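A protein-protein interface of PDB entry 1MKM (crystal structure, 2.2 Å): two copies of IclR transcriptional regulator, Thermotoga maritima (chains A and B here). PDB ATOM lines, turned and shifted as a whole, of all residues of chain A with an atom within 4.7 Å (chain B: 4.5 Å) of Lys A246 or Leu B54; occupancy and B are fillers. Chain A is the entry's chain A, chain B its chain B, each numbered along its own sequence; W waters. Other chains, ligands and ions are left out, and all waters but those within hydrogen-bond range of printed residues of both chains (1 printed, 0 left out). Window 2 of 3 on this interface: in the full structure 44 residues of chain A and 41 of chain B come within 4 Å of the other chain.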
ATOM      1  N   PHE A  78     -29.691  26.785 -15.832  1.00  0.00           N
ATOM      2  CA  PHE A  78     -29.144  25.944 -14.778  1.00  0.00           C
ATOM      3  C   PHE A  78     -30.040  24.709 -14.691  1.00  0.00           C
ATOM      4  O   PHE A  78     -31.247  24.819 -14.813  1.00  0.00           O
ATOM      5  CB  PHE A  78     -29.131  26.693 -13.457  1.00  0.00           C
ATOM      6  CG  PHE A  78     -27.939  26.390 -12.599  1.00  0.00           C
ATOM      7  CD1 PHE A  78     -26.653  26.739 -13.018  1.00  0.00           C
ATOM      8  CD2 PHE A  78     -28.094  25.819 -11.340  1.00  0.00           C
ATOM      9  CE1 PHE A  78     -25.541  26.532 -12.192  1.00  0.00           C
ATOM     10  CE2 PHE A  78     -26.982  25.608 -10.506  1.00  0.00           C
ATOM     11  CZ  PHE A  78     -25.708  25.971 -10.942  1.00  0.00           C
ATOM     12  N   ILE A  83     -27.656  18.165 -11.877  1.00  0.00           N
ATOM     13  CA  ILE A  83     -26.840  18.352 -10.678  1.00  0.00           C
ATOM     14  C   ILE A  83     -27.193  17.369  -9.560  1.00  0.00           C
ATOM     15  O   ILE A  83     -26.314  16.854  -8.880  1.00  0.00           O
ATOM     16  CB  ILE A  83     -27.025  19.787 -10.110  1.00  0.00           C
ATOM     17  CG1 ILE A  83     -26.327  20.801 -11.019  1.00  0.00           C
ATOM     18  CG2 ILE A  83     -26.530  19.856  -8.667  1.00  0.00           C
ATOM     19  CD1 ILE A  83     -26.696  22.239 -10.715  1.00  0.00           C
ATOM     20  N   HIS A  87     -27.279  12.021  -6.850  1.00  0.00           N
ATOM     21  CA  HIS A  87     -27.614  12.008  -5.438  1.00  0.00           C
ATOM     22  C   HIS A  87     -28.934  11.251  -5.310  1.00  0.00           C
ATOM     23  O   HIS A  87     -29.095  10.411  -4.420  1.00  0.00           O
ATOM     24  CB  HIS A  87     -27.772  13.428  -4.900  1.00  0.00           C
ATOM     25  CG  HIS A  87     -26.484  14.180  -4.784  1.00  0.00           C
ATOM     26  ND1 HIS A  87     -25.745  14.566  -5.881  1.00  0.00           N
ATOM     27  CD2 HIS A  87     -25.814  14.633  -3.700  1.00  0.00           C
ATOM     28  CE1 HIS A  87     -24.674  15.226  -5.476  1.00  0.00           C
ATOM     29  NE2 HIS A  87     -24.693  15.281  -4.157  1.00  0.00           N
ATOM     30  N   GLU A 242     -25.997  18.600   0.174  1.00  0.00           N
ATOM     31  CA  GLU A 242     -25.035  18.536  -0.921  1.00  0.00           C
ATOM     32  C   GLU A 242     -25.542  19.268  -2.152  1.00  0.00           C
ATOM     33  O   GLU A 242     -24.823  20.084  -2.729  1.00  0.00           O
ATOM     34  CB  GLU A 242     -24.714  17.079  -1.272  1.00  0.00           C
ATOM     35  CG  GLU A 242     -23.584  16.486  -0.438  1.00  0.00           C
ATOM     36  CD  GLU A 242     -23.443  14.984  -0.601  1.00  0.00           C
ATOM     37  OE1 GLU A 242     -23.422  14.505  -1.756  1.00  0.00           O
ATOM     38  OE2 GLU A 242     -23.342  14.283   0.430  1.00  0.00           O
ATOM     39  N   ILE A 243     -26.783  18.985  -2.550  1.00  0.00           N
ATOM     40  CA  ILE A 243     -27.372  19.632  -3.720  1.00  0.00           C
ATOM     41  C   ILE A 243     -27.460  21.143  -3.519  1.00  0.00           C
ATOM     42  O   ILE A 243     -26.951  21.917  -4.330  1.00  0.00           O
ATOM     43  CB  ILE A 243     -28.785  19.082  -4.019  1.00  0.00           C
ATOM     44  CG1 ILE A 243     -28.715  17.563  -4.236  1.00  0.00           C
ATOM     45  CG2 ILE A 243     -29.360  19.762  -5.258  1.00  0.00           C
ATOM     46  CD1 ILE A 243     -30.047  16.901  -4.510  1.00  0.00           C
ATOM     47  N   SER A 244     -28.098  21.564  -2.431  1.00  0.00           N
ATOM     48  CA  SER A 244     -28.246  22.983  -2.143  1.00  0.00           C
ATOM     49  C   SER A 244     -26.900  23.697  -2.047  1.00  0.00           C
ATOM     50  O   SER A 244     -26.779  24.856  -2.440  1.00  0.00           O
ATOM     51  CB  SER A 244     -29.030  23.176  -0.850  1.00  0.00           C
ATOM     52  OG  SER A 244     -30.335  22.646  -0.987  1.00  0.00           O
ATOM     53  N   ARG A 245     -25.892  23.003  -1.531  1.00  0.00           N
ATOM     54  CA  ARG A 245     -24.568  23.592  -1.403  1.00  0.00           C
ATOM     55  C   ARG A 245     -23.993  23.848  -2.784  1.00  0.00           C
ATOM     56  O   ARG A 245     -23.294  24.837  -2.993  1.00  0.00           O
ATOM     57  CB  ARG A 245     -23.645  22.668  -0.616  1.00  0.00           C
ATOM     58  CG  ARG A 245     -22.348  23.318  -0.180  1.00  0.00           C
ATOM     59  CD  ARG A 245     -21.550  22.351   0.668  1.00  0.00           C
ATOM     60  NE  ARG A 245     -21.299  21.108  -0.059  1.00  0.00           N
ATOM     61  CZ  ARG A 245     -21.409  19.891   0.467  1.00  0.00           C
ATOM     62  NH1 ARG A 245     -21.768  19.740   1.736  1.00  0.00           N
ATOM     63  NH2 ARG A 245     -21.170  18.823  -0.285  1.00  0.00           N
ATOM     64  N   LYS A 246     -24.292  22.953  -3.724  1.00  0.00           N
ATOM     65  CA  LYS A 246     -23.811  23.101  -5.096  1.00  0.00           C
ATOM     66  C   LYS A 246     -24.616  24.169  -5.834  1.00  0.00           C
ATOM     67  O   LYS A 246     -24.290  24.535  -6.962  1.00  0.00           O
ATOM     68  CB  LYS A 246     -23.889  21.767  -5.850  1.00  0.00           C
ATOM     69  CG  LYS A 246     -22.939  20.705  -5.311  1.00  0.00           C
ATOM     70  CD  LYS A 246     -23.021  19.394  -6.084  1.00  0.00           C
ATOM     71  CE  LYS A 246     -22.380  19.492  -7.460  1.00  0.00           C
ATOM     72  NZ  LYS A 246     -22.433  18.188  -8.181  1.00  0.00           N
ATOM     73  N   LEU A 247     -25.674  24.659  -5.197  1.00  0.00           N
ATOM     74  CA  LEU A 247     -26.499  25.707  -5.787  1.00  0.00           C
ATOM     75  C   LEU A 247     -26.034  27.031  -5.183  1.00  0.00           C
ATOM     76  O   LEU A 247     -26.581  28.099  -5.474  1.00  0.00           O
ATOM     77  CB  LEU A 247     -27.986  25.483  -5.472  1.00  0.00           C
ATOM     78  CG  LEU A 247     -28.663  24.221  -6.011  1.00  0.00           C
ATOM     79  CD1 LEU A 247     -30.162  24.302  -5.742  1.00  0.00           C
ATOM     80  CD2 LEU A 247     -28.388  24.078  -7.504  1.00  0.00           C
ATOM     81  N   GLY A 248     -25.017  26.943  -4.329  1.00  0.00           N
ATOM     82  CA  GLY A 248     -24.477  28.127  -3.692  1.00  0.00           C
ATOM     83  C   GLY A 248     -24.965  28.384  -2.279  1.00  0.00           C
ATOM     84  O   GLY A 248     -24.674  29.432  -1.707  1.00  0.00           O
ATOM     85  N   VAL B  53     -17.644  27.936 -12.123  1.00  0.00           N
ATOM     86  CA  VAL B  53     -17.857  26.752 -12.920  1.00  0.00           C
ATOM     87  C   VAL B  53     -18.106  25.549 -12.023  1.00  0.00           C
ATOM     88  O   VAL B  53     -17.681  25.524 -10.861  1.00  0.00           O
ATOM     89  CB  VAL B  53     -16.641  26.507 -13.821  1.00  0.00           C
ATOM     90  CG1 VAL B  53     -16.739  25.177 -14.480  1.00  0.00           C
ATOM     91  CG2 VAL B  53     -16.572  27.601 -14.868  1.00  0.00           C
ATOM     92  N   LEU B  54     -18.813  24.560 -12.559  1.00  0.00           N
ATOM     93  CA  LEU B  54     -19.118  23.339 -11.815  1.00  0.00           C
ATOM     94  C   LEU B  54     -18.488  22.174 -12.545  1.00  0.00           C
ATOM     95  O   LEU B  54     -18.598  22.069 -13.773  1.00  0.00           O
ATOM     96  CB  LEU B  54     -20.633  23.130 -11.728  1.00  0.00           C
ATOM     97  CG  LEU B  54     -21.115  22.084 -10.716  1.00  0.00           C
ATOM     98  CD1 LEU B  54     -20.572  22.435  -9.335  1.00  0.00           C
ATOM     99  CD2 LEU B  54     -22.656  22.042 -10.703  1.00  0.00           C
ATOM    100  N   ARG B  55     -17.803  21.301 -11.820  1.00  0.00           N
ATOM    101  CA  ARG B  55     -17.214  20.176 -12.522  1.00  0.00           C
ATOM    102  C   ARG B  55     -18.043  18.925 -12.312  1.00  0.00           C
ATOM    103  O   ARG B  55     -18.383  18.575 -11.181  1.00  0.00           O
ATOM    104  CB  ARG B  55     -15.753  19.929 -12.118  1.00  0.00           C
ATOM    105  CG  ARG B  55     -15.053  19.080 -13.162  1.00  0.00           C
ATOM    106  CD  ARG B  55     -13.568  18.891 -12.928  1.00  0.00           C
ATOM    107  NE  ARG B  55     -12.941  18.279 -14.099  1.00  0.00           N
ATOM    108  CZ  ARG B  55     -11.639  18.017 -14.204  1.00  0.00           C
ATOM    109  NH1 ARG B  55     -10.816  18.306 -13.203  1.00  0.00           N
ATOM    110  NH2 ARG B  55     -11.157  17.482 -15.326  1.00  0.00           N
ATOM    111  N   LYS B  56     -18.371  18.278 -13.428  1.00  0.00           N
ATOM    112  CA  LYS B  56     -19.177  17.063 -13.453  1.00  0.00           C
ATOM    113  C   LYS B  56     -18.408  15.818 -13.026  1.00  0.00           C
ATOM    114  O   LYS B  56     -17.168  15.798 -13.016  1.00  0.00           O
ATOM    115  CB  LYS B  56     -19.723  16.822 -14.865  1.00  0.00           C
ATOM    116  CG  LYS B  56     -20.609  17.920 -15.432  1.00  0.00           C
ATOM    117  CD  LYS B  56     -21.098  17.534 -16.827  1.00  0.00           C
ATOM    118  CE  LYS B  56     -22.122  18.526 -17.361  1.00  0.00           C
ATOM    119  NZ  LYS B  56     -22.815  18.039 -18.589  1.00  0.00           N
ATOM    120  N   ARG B  60     -16.298  16.952 -16.943  1.00  0.00           N
ATOM    121  CA  ARG B  60     -16.649  17.973 -17.929  1.00  0.00           C
ATOM    122  C   ARG B  60     -17.155  19.163 -17.111  1.00  0.00           C
ATOM    123  O   ARG B  60     -17.630  18.986 -15.986  1.00  0.00           O
ATOM    124  CB  ARG B  60     -17.751  17.472 -18.861  1.00  0.00           C
ATOM    125  CG  ARG B  60     -17.430  16.158 -19.541  1.00  0.00           C
ATOM    126  CD  ARG B  60     -16.565  16.351 -20.757  1.00  0.00           C
ATOM    127  NE  ARG B  60     -17.307  17.025 -21.811  1.00  0.00           N
ATOM    128  CZ  ARG B  60     -16.844  17.201 -23.042  1.00  0.00           C
ATOM    129  NH1 ARG B  60     -15.639  16.746 -23.368  1.00  0.00           N
ATOM    130  NH2 ARG B  60     -17.585  17.830 -23.946  1.00  0.00           N
ATOM    131  N   TYR B  61     -17.075  20.362 -17.685  1.00  0.00           N
ATOM    132  CA  TYR B  61     -17.464  21.584 -16.985  1.00  0.00           C
ATOM    133  C   TYR B  61     -18.771  22.285 -17.382  1.00  0.00           C
ATOM    134  O   TYR B  61     -19.117  22.400 -18.553  1.00  0.00           O
ATOM    135  CB  TYR B  61     -16.335  22.608 -17.086  1.00  0.00           C
ATOM    136  CG  TYR B  61     -15.065  22.240 -16.346  1.00  0.00           C
ATOM    137  CD1 TYR B  61     -14.066  21.480 -16.960  1.00  0.00           C
ATOM    138  CD2 TYR B  61     -14.850  22.688 -15.046  1.00  0.00           C
ATOM    139  CE1 TYR B  61     -12.875  21.184 -16.288  1.00  0.00           C
ATOM    140  CE2 TYR B  61     -13.668  22.398 -14.368  1.00  0.00           C
ATOM    141  CZ  TYR B  61     -12.687  21.653 -14.994  1.00  0.00           C
ATOM    142  OH  TYR B  61     -11.515  21.410 -14.329  1.00  0.00           O
ATOM    143  N   VAL B  62     -19.449  22.799 -16.366  1.00  0.00           N
ATOM    144  CA  VAL B  62     -20.705  23.501 -16.538  1.00  0.00           C
ATOM    145  C   VAL B  62     -20.660  24.757 -15.675  1.00  0.00           C
ATOM    146  O   VAL B  62     -19.974  24.794 -14.653  1.00  0.00           O
ATOM    147  CB  VAL B  62     -21.875  22.565 -16.126  1.00  0.00           C
ATOM    148  CG1 VAL B  62     -22.840  23.271 -15.223  1.00  0.00           C
ATOM    149  CG2 VAL B  62     -22.572  22.042 -17.369  1.00  0.00           C
ATOM    150  N   PRO B  63     -21.369  25.816 -16.085  1.00  0.00           N
ATOM    151  CA  PRO B  63     -21.348  27.041 -15.279  1.00  0.00           C
ATOM    152  C   PRO B  63     -21.847  26.860 -13.848  1.00  0.00           C
ATOM    153  O   PRO B  63     -22.790  26.113 -13.588  1.00  0.00           O
ATOM    154  CB  PRO B  63     -22.208  28.020 -16.092  1.00  0.00           C
ATOM    155  CG  PRO B  63     -23.072  27.130 -16.925  1.00  0.00           C
ATOM    156  CD  PRO B  63     -22.152  26.007 -17.315  1.00  0.00           C
ATOM    157  N   GLY B  64     -21.190  27.559 -12.929  1.00  0.00           N
ATOM    158  CA  GLY B  64     -21.542  27.498 -11.526  1.00  0.00           C
ATOM    159  C   GLY B  64     -22.631  28.476 -11.136  1.00  0.00           C
ATOM    160  O   GLY B  64     -23.237  29.133 -11.983  1.00  0.00           O
ATOM    161  N   TYR B  65     -22.859  28.583  -9.835  1.00  0.00           N
ATOM    162  CA  TYR B  65     -23.891  29.442  -9.281  1.00  0.00           C
ATOM    163  C   TYR B  65     -23.408  30.850  -8.979  1.00  0.00           C
ATOM    164  O   TYR B  65     -24.213  31.766  -8.868  1.00  0.00           O
ATOM    165  CB  TYR B  65     -24.397  28.829  -7.979  1.00  0.00           C
ATOM    166  CG  TYR B  65     -23.496  29.170  -6.815  1.00  0.00           C
ATOM    167  CD1 TYR B  65     -23.725  30.316  -6.046  1.00  0.00           C
ATOM    168  CD2 TYR B  65     -22.353  28.417  -6.547  1.00  0.00           C
ATOM    169  CE1 TYR B  65     -22.845  30.706  -5.052  1.00  0.00           C
ATOM    170  CE2 TYR B  65     -21.453  28.805  -5.547  1.00  0.00           C
ATOM    171  CZ  TYR B  65     -21.709  29.950  -4.809  1.00  0.00           C
ATOM    172  OH  TYR B  65     -20.830  30.356  -3.830  1.00  0.00           O
HETATM  173  O   HOH W   1     -20.408  18.045  -9.710  1.00  0.00           O
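Among the printed residues, pairs that only touch across the chains: Phe A78 with Pro B63 (3.1 Å), Phe A78 with Gly B64 (3.5 Å), Ile A83 with Leu B54 (3.9 Å), Lys A246 with Leu B54 (3.9 Å), Leu A247 with Tyr B65 (3.4 Å) and Gly A248 with Tyr B65 (3.3 Å).
Water W1 bridges NZ of Lys A246 (2.5 Å) and O of Arg B55 (2.6 Å).
No position is printed for both chains.
Of the 6 pairs that touch across the chains among the printed residues, none has its exchanged pair printed and touching as well.
Hydrophobic or aromatic side chains of chain B within 4 Å of the printed part of chain A: Leu B54 and Tyr B65.
Among the printed residues, no Asp or Glu carboxylate lies within 4 Å of a Lys or Arg side-chain nitrogen of the other chain.
The backbone NH of Leu B54 sits at hydrogen-bond distance from the backbone carbonyl oxygen of Val B62.
Printed residues of chain B within 4 Å of Lys A246: Leu B54 (3.9 Å).
Of chain A, only Ile A83 (3.9 Å) and Lys A246 (3.9 Å) come within 4 Å of Leu B54.
Printed residues of chain B within 4 Å of Phe A78: Pro B63 and Gly B64.
Of the printed residues of chain A, Pro B63 touches Phe A78.
Of the printed residues of chain B, Leu A247 touches Tyr B65 (3.4 Å).
Of the printed residues of chain A, Tyr B65 touches Leu A247 (3.4 Å) and Gly A248 (3.3 Å).
The nearest printed residue of chain A that does not touch Leu B54 is Phe A78 (5.0 Å).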
